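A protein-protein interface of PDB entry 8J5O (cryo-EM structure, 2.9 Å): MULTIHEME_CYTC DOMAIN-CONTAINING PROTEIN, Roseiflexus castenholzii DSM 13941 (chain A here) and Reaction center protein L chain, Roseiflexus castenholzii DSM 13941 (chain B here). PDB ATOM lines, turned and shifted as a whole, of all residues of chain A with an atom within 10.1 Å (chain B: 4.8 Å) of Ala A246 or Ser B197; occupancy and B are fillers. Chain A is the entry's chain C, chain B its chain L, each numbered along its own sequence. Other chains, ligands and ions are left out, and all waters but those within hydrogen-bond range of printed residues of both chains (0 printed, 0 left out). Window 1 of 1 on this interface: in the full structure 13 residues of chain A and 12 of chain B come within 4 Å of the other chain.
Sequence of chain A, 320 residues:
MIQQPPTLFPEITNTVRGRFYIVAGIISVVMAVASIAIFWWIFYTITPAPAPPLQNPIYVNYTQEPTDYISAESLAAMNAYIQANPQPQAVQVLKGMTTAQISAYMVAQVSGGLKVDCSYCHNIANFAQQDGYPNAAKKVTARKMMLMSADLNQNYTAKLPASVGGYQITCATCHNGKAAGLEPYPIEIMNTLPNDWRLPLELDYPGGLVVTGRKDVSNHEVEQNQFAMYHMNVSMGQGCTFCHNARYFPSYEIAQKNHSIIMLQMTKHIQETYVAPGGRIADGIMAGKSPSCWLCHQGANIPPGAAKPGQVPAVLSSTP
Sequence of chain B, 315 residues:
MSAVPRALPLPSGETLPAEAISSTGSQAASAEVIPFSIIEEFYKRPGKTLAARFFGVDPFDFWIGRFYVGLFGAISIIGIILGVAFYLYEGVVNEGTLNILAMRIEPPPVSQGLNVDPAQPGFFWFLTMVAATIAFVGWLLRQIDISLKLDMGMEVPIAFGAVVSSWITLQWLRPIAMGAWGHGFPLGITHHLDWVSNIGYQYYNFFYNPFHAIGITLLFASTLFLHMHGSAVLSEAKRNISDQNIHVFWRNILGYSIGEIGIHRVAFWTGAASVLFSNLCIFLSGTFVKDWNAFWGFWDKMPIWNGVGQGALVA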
ATOM      1  N   THR A 212     -19.583 -35.956 -29.612  1.00  0.00           N
ATOM      2  CA  THR A 212     -18.682 -34.818 -29.789  1.00  0.00           C
ATOM      3  C   THR A 212     -17.754 -35.050 -30.976  1.00  0.00           C
ATOM      4  O   THR A 212     -16.894 -35.936 -30.941  1.00  0.00           O
ATOM      5  CB  THR A 212     -17.881 -34.573 -28.516  1.00  0.00           C
ATOM      6  OG1 THR A 212     -18.778 -34.292 -27.435  1.00  0.00           O
ATOM      7  CG2 THR A 212     -16.939 -33.400 -28.702  1.00  0.00           C
ATOM      8  N   GLY A 239     -28.138 -31.341 -10.713  1.00  0.00           N
ATOM      9  CA  GLY A 239     -27.877 -30.575 -11.913  1.00  0.00           C
ATOM     10  C   GLY A 239     -26.849 -31.230 -12.813  1.00  0.00           C
ATOM     11  O   GLY A 239     -26.277 -32.279 -12.519  1.00  0.00           O
ATOM     12  N   CYS A 240     -26.596 -30.561 -13.938  1.00  0.00           N
ATOM     13  CA  CYS A 240     -25.837 -31.170 -15.025  1.00  0.00           C
ATOM     14  C   CYS A 240     -24.352 -31.285 -14.713  1.00  0.00           C
ATOM     15  O   CYS A 240     -23.654 -32.055 -15.378  1.00  0.00           O
ATOM     16  CB  CYS A 240     -26.046 -30.362 -16.305  1.00  0.00           C
ATOM     17  SG  CYS A 240     -25.602 -31.209 -17.809  1.00  0.00           S
ATOM     18  N   THR A 241     -23.861 -30.553 -13.722  1.00  0.00           N
ATOM     19  CA  THR A 241     -22.457 -30.586 -13.338  1.00  0.00           C
ATOM     20  C   THR A 241     -22.133 -31.703 -12.354  1.00  0.00           C
ATOM     21  O   THR A 241     -20.967 -31.865 -11.997  1.00  0.00           O
ATOM     22  CB  THR A 241     -22.033 -29.227 -12.745  1.00  0.00           C
ATOM     23  OG1 THR A 241     -22.804 -28.933 -11.578  1.00  0.00           O
ATOM     24  CG2 THR A 241     -22.197 -28.099 -13.760  1.00  0.00           C
ATOM     25  N   PHE A 242     -23.116 -32.513 -11.950  1.00  0.00           N
ATOM     26  CA  PHE A 242     -22.852 -33.556 -10.963  1.00  0.00           C
ATOM     27  C   PHE A 242     -21.802 -34.546 -11.461  1.00  0.00           C
ATOM     28  O   PHE A 242     -20.928 -34.972 -10.698  1.00  0.00           O
ATOM     29  CB  PHE A 242     -24.153 -34.270 -10.594  1.00  0.00           C
ATOM     30  CG  PHE A 242     -24.021 -35.183  -9.417  1.00  0.00           C
ATOM     31  CD1 PHE A 242     -23.552 -34.693  -8.218  1.00  0.00           C
ATOM     32  CD2 PHE A 242     -24.326 -36.529  -9.515  1.00  0.00           C
ATOM     33  CE1 PHE A 242     -23.409 -35.514  -7.127  1.00  0.00           C
ATOM     34  CE2 PHE A 242     -24.190 -37.360  -8.416  1.00  0.00           C
ATOM     35  CZ  PHE A 242     -23.724 -36.847  -7.224  1.00  0.00           C
ATOM     36  N   CYS A 243     -21.857 -34.904 -12.741  1.00  0.00           N
ATOM     37  CA  CYS A 243     -20.907 -35.829 -13.337  1.00  0.00           C
ATOM     38  C   CYS A 243     -20.013 -35.201 -14.396  1.00  0.00           C
ATOM     39  O   CYS A 243     -19.138 -35.895 -14.924  1.00  0.00           O
ATOM     40  CB  CYS A 243     -21.649 -37.023 -13.952  1.00  0.00           C
ATOM     41  SG  CYS A 243     -23.033 -37.643 -12.975  1.00  0.00           S
ATOM     42  N   HIS A 244     -20.187 -33.921 -14.720  1.00  0.00           N
ATOM     43  CA  HIS A 244     -19.542 -33.320 -15.878  1.00  0.00           C
ATOM     44  C   HIS A 244     -18.804 -32.045 -15.492  1.00  0.00           C
ATOM     45  O   HIS A 244     -19.031 -31.456 -14.433  1.00  0.00           O
ATOM     46  CB  HIS A 244     -20.567 -32.994 -16.975  1.00  0.00           C
ATOM     47  CG  HIS A 244     -20.888 -34.147 -17.874  1.00  0.00           C
ATOM     48  ND1 HIS A 244     -19.959 -34.726 -18.709  1.00  0.00           N
ATOM     49  CD2 HIS A 244     -22.041 -34.826 -18.069  1.00  0.00           C
ATOM     50  CE1 HIS A 244     -20.526 -35.714 -19.376  1.00  0.00           C
ATOM     51  NE2 HIS A 244     -21.790 -35.794 -19.009  1.00  0.00           N
ATOM     52  N   ASN A 245     -17.902 -31.631 -16.377  1.00  0.00           N
ATOM     53  CA  ASN A 245     -17.357 -30.279 -16.407  1.00  0.00           C
ATOM     54  C   ASN A 245     -17.816 -29.645 -17.712  1.00  0.00           C
ATOM     55  O   ASN A 245     -17.525 -30.169 -18.792  1.00  0.00           O
ATOM     56  CB  ASN A 245     -15.831 -30.289 -16.305  1.00  0.00           C
ATOM     57  CG  ASN A 245     -15.246 -28.900 -16.125  1.00  0.00           C
ATOM     58  OD1 ASN A 245     -15.967 -27.906 -16.101  1.00  0.00           O
ATOM     59  ND2 ASN A 245     -13.929 -28.827 -15.995  1.00  0.00           N
ATOM     60  N   ALA A 246     -18.536 -28.526 -17.616  1.00  0.00           N
ATOM     61  CA  ALA A 246     -19.233 -28.003 -18.785  1.00  0.00           C
ATOM     62  C   ALA A 246     -18.274 -27.444 -19.830  1.00  0.00           C
ATOM     63  O   ALA A 246     -18.666 -27.248 -20.984  1.00  0.00           O
ATOM     64  CB  ALA A 246     -20.242 -26.937 -18.361  1.00  0.00           C
ATOM     65  N   ARG A 247     -17.021 -27.180 -19.454  1.00  0.00           N
ATOM     66  CA  ARG A 247     -16.054 -26.686 -20.428  1.00  0.00           C
ATOM     67  C   ARG A 247     -15.722 -27.753 -21.466  1.00  0.00           C
ATOM     68  O   ARG A 247     -15.497 -27.435 -22.639  1.00  0.00           O
ATOM     69  CB  ARG A 247     -14.788 -26.206 -19.717  1.00  0.00           C
ATOM     70  CG  ARG A 247     -14.046 -27.301 -18.984  1.00  0.00           C
ATOM     71  CD  ARG A 247     -12.812 -26.788 -18.267  1.00  0.00           C
ATOM     72  NE  ARG A 247     -11.766 -26.329 -19.169  1.00  0.00           N
ATOM     73  CZ  ARG A 247     -10.730 -25.595 -18.789  1.00  0.00           C
ATOM     74  NH1 ARG A 247     -10.571 -25.223 -17.532  1.00  0.00           N
ATOM     75  NH2 ARG A 247      -9.829 -25.227 -19.692  1.00  0.00           N
ATOM     76  N   TYR A 248     -15.684 -29.022 -21.056  1.00  0.00           N
ATOM     77  CA  TYR A 248     -15.424 -30.126 -21.979  1.00  0.00           C
ATOM     78  C   TYR A 248     -16.208 -31.337 -21.478  1.00  0.00           C
ATOM     79  O   TYR A 248     -15.834 -31.948 -20.474  1.00  0.00           O
ATOM     80  CB  TYR A 248     -13.936 -30.429 -22.074  1.00  0.00           C
ATOM     81  CG  TYR A 248     -13.553 -31.242 -23.288  1.00  0.00           C
ATOM     82  CD1 TYR A 248     -14.088 -30.953 -24.536  1.00  0.00           C
ATOM     83  CD2 TYR A 248     -12.663 -32.299 -23.186  1.00  0.00           C
ATOM     84  CE1 TYR A 248     -13.741 -31.689 -25.646  1.00  0.00           C
ATOM     85  CE2 TYR A 248     -12.312 -33.043 -24.292  1.00  0.00           C
ATOM     86  CZ  TYR A 248     -12.854 -32.732 -25.521  1.00  0.00           C
ATOM     87  OH  TYR A 248     -12.509 -33.468 -26.628  1.00  0.00           O
ATOM     88  N   PHE A 249     -17.293 -31.666 -22.173  1.00  0.00           N
ATOM     89  CA  PHE A 249     -18.106 -32.814 -21.779  1.00  0.00           C
ATOM     90  C   PHE A 249     -17.396 -34.161 -21.885  1.00  0.00           C
ATOM     91  O   PHE A 249     -17.604 -35.000 -20.992  1.00  0.00           O
ATOM     92  CB  PHE A 249     -19.413 -32.817 -22.582  1.00  0.00           C
ATOM     93  CG  PHE A 249     -20.408 -31.799 -22.108  1.00  0.00           C
ATOM     94  CD1 PHE A 249     -20.989 -31.913 -20.860  1.00  0.00           C
ATOM     95  CD2 PHE A 249     -20.751 -30.720 -22.901  1.00  0.00           C
ATOM     96  CE1 PHE A 249     -21.897 -30.978 -20.416  1.00  0.00           C
ATOM     97  CE2 PHE A 249     -21.660 -29.782 -22.460  1.00  0.00           C
ATOM     98  CZ  PHE A 249     -22.231 -29.911 -21.216  1.00  0.00           C
ATOM     99  N   PRO A 250     -16.593 -34.455 -22.916  1.00  0.00           N
ATOM    100  CA  PRO A 250     -15.949 -35.780 -22.987  1.00  0.00           C
ATOM    101  C   PRO A 250     -14.975 -36.086 -21.854  1.00  0.00           C
ATOM    102  O   PRO A 250     -14.550 -37.242 -21.738  1.00  0.00           O
ATOM    103  CB  PRO A 250     -15.221 -35.742 -24.335  1.00  0.00           C
ATOM    104  CG  PRO A 250     -15.990 -34.786 -25.140  1.00  0.00           C
ATOM    105  CD  PRO A 250     -16.452 -33.729 -24.192  1.00  0.00           C
ATOM    106  N   SER A 251     -14.609 -35.113 -21.025  1.00  0.00           N
ATOM    107  CA  SER A 251     -13.615 -35.341 -19.986  1.00  0.00           C
ATOM    108  C   SER A 251     -14.124 -36.309 -18.919  1.00  0.00           C
ATOM    109  O   SER A 251     -15.313 -36.347 -18.595  1.00  0.00           O
ATOM    110  CB  SER A 251     -13.220 -34.015 -19.338  1.00  0.00           C
ATOM    111  OG  SER A 251     -12.117 -34.182 -18.468  1.00  0.00           O
ATOM    112  N   GLU A 253     -13.231 -36.606 -15.284  1.00  0.00           N
ATOM    113  CA  GLU A 253     -12.511 -36.008 -14.167  1.00  0.00           C
ATOM    114  C   GLU A 253     -13.330 -35.813 -12.899  1.00  0.00           C
ATOM    115  O   GLU A 253     -12.740 -35.509 -11.858  1.00  0.00           O
ATOM    116  CB  GLU A 253     -11.924 -34.649 -14.575  1.00  0.00           C
ATOM    117  CG  GLU A 253     -12.971 -33.601 -14.891  1.00  0.00           C
ATOM    118  CD  GLU A 253     -12.363 -32.296 -15.348  1.00  0.00           C
ATOM    119  OE1 GLU A 253     -11.122 -32.216 -15.439  1.00  0.00           O
ATOM    120  OE2 GLU A 253     -13.126 -31.347 -15.615  1.00  0.00           O
ATOM    121  N   ILE A 254     -14.657 -35.971 -12.942  1.00  0.00           N
ATOM    122  CA  ILE A 254     -15.480 -35.682 -11.769  1.00  0.00           C
ATOM    123  C   ILE A 254     -15.679 -36.901 -10.878  1.00  0.00           C
ATOM    124  O   ILE A 254     -16.055 -36.745  -9.706  1.00  0.00           O
ATOM    125  CB  ILE A 254     -16.827 -35.080 -12.216  1.00  0.00           C
ATOM    126  CG1 ILE A 254     -16.579 -33.802 -13.014  1.00  0.00           C
ATOM    127  CG2 ILE A 254     -17.698 -34.742 -11.026  1.00  0.00           C
ATOM    128  CD1 ILE A 254     -15.870 -32.724 -12.234  1.00  0.00           C
ATOM    129  N   LYS A 257     -18.752 -40.088 -13.117  1.00  0.00           N
ATOM    130  CA  LYS A 257     -19.091 -40.507 -14.469  1.00  0.00           C
ATOM    131  C   LYS A 257     -18.760 -41.980 -14.699  1.00  0.00           C
ATOM    132  O   LYS A 257     -19.502 -42.678 -15.402  1.00  0.00           O
ATOM    133  CB  LYS A 257     -18.378 -39.593 -15.467  1.00  0.00           C
ATOM    134  CG  LYS A 257     -18.716 -39.823 -16.923  1.00  0.00           C
ATOM    135  CD  LYS A 257     -18.011 -38.797 -17.794  1.00  0.00           C
ATOM    136  CE  LYS A 257     -18.324 -39.002 -19.258  1.00  0.00           C
ATOM    137  NZ  LYS A 257     -17.637 -38.006 -20.117  1.00  0.00           N
ATOM    138  N   LEU B 193     -15.195 -17.392 -18.946  1.00  0.00           N
ATOM    139  CA  LEU B 193     -16.077 -18.176 -19.800  1.00  0.00           C
ATOM    140  C   LEU B 193     -16.313 -19.566 -19.221  1.00  0.00           C
ATOM    141  O   LEU B 193     -17.405 -20.126 -19.364  1.00  0.00           O
ATOM    142  CB  LEU B 193     -15.468 -18.270 -21.195  1.00  0.00           C
ATOM    143  CG  LEU B 193     -15.383 -16.927 -21.922  1.00  0.00           C
ATOM    144  CD1 LEU B 193     -14.648 -17.073 -23.241  1.00  0.00           C
ATOM    145  CD2 LEU B 193     -16.759 -16.354 -22.117  1.00  0.00           C
ATOM    146  N   ASP B 194     -15.301 -20.137 -18.565  1.00  0.00           N
ATOM    147  CA  ASP B 194     -15.473 -21.414 -17.879  1.00  0.00           C
ATOM    148  C   ASP B 194     -16.518 -21.301 -16.778  1.00  0.00           C
ATOM    149  O   ASP B 194     -17.385 -22.171 -16.629  1.00  0.00           O
ATOM    150  CB  ASP B 194     -14.136 -21.869 -17.296  1.00  0.00           C
ATOM    151  CG  ASP B 194     -13.187 -22.397 -18.346  1.00  0.00           C
ATOM    152  OD1 ASP B 194     -13.439 -22.179 -19.547  1.00  0.00           O
ATOM    153  OD2 ASP B 194     -12.172 -23.014 -17.968  1.00  0.00           O
ATOM    154  N   TRP B 195     -16.443 -20.225 -15.992  1.00  0.00           N
ATOM    155  CA  TRP B 195     -17.433 -19.988 -14.948  1.00  0.00           C
ATOM    156  C   TRP B 195     -18.824 -19.812 -15.541  1.00  0.00           C
ATOM    157  O   TRP B 195     -19.799 -20.362 -15.019  1.00  0.00           O
ATOM    158  CB  TRP B 195     -17.036 -18.761 -14.123  1.00  0.00           C
ATOM    159  CG  TRP B 195     -17.977 -18.424 -13.000  1.00  0.00           C
ATOM    160  CD1 TRP B 195     -17.917 -18.882 -11.718  1.00  0.00           C
ATOM    161  CD2 TRP B 195     -19.105 -17.538 -13.054  1.00  0.00           C
ATOM    162  NE1 TRP B 195     -18.939 -18.348 -10.973  1.00  0.00           N
ATOM    163  CE2 TRP B 195     -19.683 -17.519 -11.770  1.00  0.00           C
ATOM    164  CE3 TRP B 195     -19.685 -16.767 -14.066  1.00  0.00           C
ATOM    165  CZ2 TRP B 195     -20.812 -16.761 -11.471  1.00  0.00           C
ATOM    166  CZ3 TRP B 195     -20.803 -16.014 -13.766  1.00  0.00           C
ATOM    167  CH2 TRP B 195     -21.355 -16.016 -12.479  1.00  0.00           C
ATOM    168  N   VAL B 196     -18.933 -19.048 -16.633  1.00  0.00           N
ATOM    169  CA  VAL B 196     -20.236 -18.851 -17.270  1.00  0.00           C
ATOM    170  C   VAL B 196     -20.808 -20.182 -17.743  1.00  0.00           C
ATOM    171  O   VAL B 196     -21.987 -20.479 -17.528  1.00  0.00           O
ATOM    172  CB  VAL B 196     -20.130 -17.841 -18.428  1.00  0.00           C
ATOM    173  CG1 VAL B 196     -21.513 -17.465 -18.928  1.00  0.00           C
ATOM    174  CG2 VAL B 196     -19.413 -16.593 -17.977  1.00  0.00           C
ATOM    175  N   SER B 197     -19.978 -21.008 -18.381  1.00  0.00           N
ATOM    176  CA  SER B 197     -20.457 -22.288 -18.894  1.00  0.00           C
ATOM    177  C   SER B 197     -20.904 -23.211 -17.765  1.00  0.00           C
ATOM    178  O   SER B 197     -21.972 -23.832 -17.844  1.00  0.00           O
ATOM    179  CB  SER B 197     -19.365 -22.948 -19.734  1.00  0.00           C
ATOM    180  OG  SER B 197     -19.714 -24.275 -20.076  1.00  0.00           O
ATOM    181  N   ASN B 198     -20.106 -23.305 -16.698  1.00  0.00           N
ATOM    182  CA  ASN B 198     -20.456 -24.198 -15.599  1.00  0.00           C
ATOM    183  C   ASN B 198     -21.703 -23.722 -14.861  1.00  0.00           C
ATOM    184  O   ASN B 198     -22.558 -24.536 -14.494  1.00  0.00           O
ATOM    185  CB  ASN B 198     -19.276 -24.339 -14.642  1.00  0.00           C
ATOM    186  CG  ASN B 198     -18.326 -25.441 -15.056  1.00  0.00           C
ATOM    187  OD1 ASN B 198     -18.521 -26.603 -14.713  1.00  0.00           O
ATOM    188  ND2 ASN B 198     -17.288 -25.080 -15.793  1.00  0.00           N
ATOM    189  N   ILE B 199     -21.830 -22.412 -14.631  1.00  0.00           N
ATOM    190  CA  ILE B 199     -23.031 -21.890 -13.986  1.00  0.00           C
ATOM    191  C   ILE B 199     -24.254 -22.106 -14.868  1.00  0.00           C
ATOM    192  O   ILE B 199     -25.332 -22.454 -14.377  1.00  0.00           O
ATOM    193  CB  ILE B 199     -22.852 -20.405 -13.621  1.00  0.00           C
ATOM    194  CG1 ILE B 199     -21.668 -20.220 -12.677  1.00  0.00           C
ATOM    195  CG2 ILE B 199     -24.111 -19.856 -12.980  1.00  0.00           C
ATOM    196  CD1 ILE B 199     -21.827 -20.949 -11.366  1.00  0.00           C
ATOM    197  N   GLY B 200     -24.110 -21.901 -16.179  1.00  0.00           N
ATOM    198  CA  GLY B 200     -25.243 -22.074 -17.069  1.00  0.00           C
ATOM    199  C   GLY B 200     -25.712 -23.512 -17.152  1.00  0.00           C
ATOM    200  O   GLY B 200     -26.912 -23.776 -17.249  1.00  0.00           O
ATOM    201  N   TYR B 201     -24.777 -24.463 -17.131  1.00  0.00           N
ATOM    202  CA  TYR B 201     -25.185 -25.860 -17.184  1.00  0.00           C
ATOM    203  C   TYR B 201     -25.552 -26.433 -15.819  1.00  0.00           C
ATOM    204  O   TYR B 201     -26.189 -27.487 -15.764  1.00  0.00           O
ATOM    205  CB  TYR B 201     -24.095 -26.711 -17.842  1.00  0.00           C
ATOM    206  CG  TYR B 201     -24.170 -26.695 -19.353  1.00  0.00           C
ATOM    207  CD1 TYR B 201     -25.175 -27.374 -20.023  1.00  0.00           C
ATOM    208  CD2 TYR B 201     -23.244 -25.990 -20.108  1.00  0.00           C
ATOM    209  CE1 TYR B 201     -25.256 -27.356 -21.400  1.00  0.00           C
ATOM    210  CE2 TYR B 201     -23.316 -25.968 -21.485  1.00  0.00           C
ATOM    211  CZ  TYR B 201     -24.325 -26.653 -22.126  1.00  0.00           C
ATOM    212  OH  TYR B 201     -24.401 -26.636 -23.499  1.00  0.00           O
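The backbone carbonyl oxygen of Phe A249 sits at hydrogen-bond distance from a ring nitrogen (ND1) of His A244, 3.3 Å away. The side-chain amide nitrogen (ND2) of Asn A245 is in hydrogen-bond range of the side-chain carboxylate (OE2) of Glu A253. O of Phe A249 lies within hydrogen-bond range of NZ of Lys A257 (3.1 Å). The backbone carbonyl oxygen (O) of Asp B194 lies within hydrogen-bond range of the side-chain amide nitrogen (ND2) of Asn B198 (3.0 Å).
Of the printed residues of chain B, Ala A246 touches Ser B197 (3.2 Å), Asn B198 (3.5 Å) and Tyr B201 (3.6 Å). Printed residues of chain A within 4 Å of Ser B197: Ala A246 (3.2 Å). No residue of chain A comes within 4 Å of Val B196. Of chain A, only Thr A241 (3.7 Å), Asn A245 (3.1 Å) and Ala A246 (3.5 Å) come within 4 Å of Asn B198. No residue of chain A comes within 4 Å of Gly B200. Of the printed residues of chain B, Phe A249 touches Tyr B201. Of the printed residues of chain A, Asp B194 touches Arg A247 (2.8 Å). Of the printed residues of chain B, Arg A247 touches Asp B194 (2.8 Å). Tyr A248 touches none of the printed residues of chain B. The nearest printed residue of chain A that does not touch Ser B197 is Arg A247 (4.01 Å). The nearest printed residue of chain B that does not touch Thr A241 is Tyr B201 (4.3 Å).
Of the 9 printed residues of chain B, 4 touch a printed residue of chain A. Hydrophobic or aromatic side chains of chain B that line the printed part of chain A: Tyr B201. Along chain B the printed residues that touch a printed residue of chain A span positions 194 to 201. Hydrophobic or aromatic side chains of chain A within 4 Å of the printed part of chain B: Ala A246 and Phe A249. Among the printed residues, 8 pairs touch across the chains.
The side-chain amide oxygen (OD1) of Asn A245 sits at hydrogen-bond distance from the side-chain amide nitrogen (ND2) of Asn B198 (3.1 Å). OG of Ser B197 lies close to O of Ala A246 (3.3 Å). The side-chain amide oxygen (OD1) of Asn B198 lies within hydrogen-bond range of the backbone NH (N) of Ala A246, at 3.5 Å. The guanidinium group (NH1) of Arg A247 lies within salt-bridge range of the side-chain carboxylate (OD2) of Asp B194.
CB of Cys A240 touches O of Tyr B201, at 2.9 Å. Thr A241 touches Asn B198. CB of Ala A246 touches CD2 of Tyr B201 (3.6 Å). Phe A249 touches Tyr B201 (CZ to CE1, 3.96 Å).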
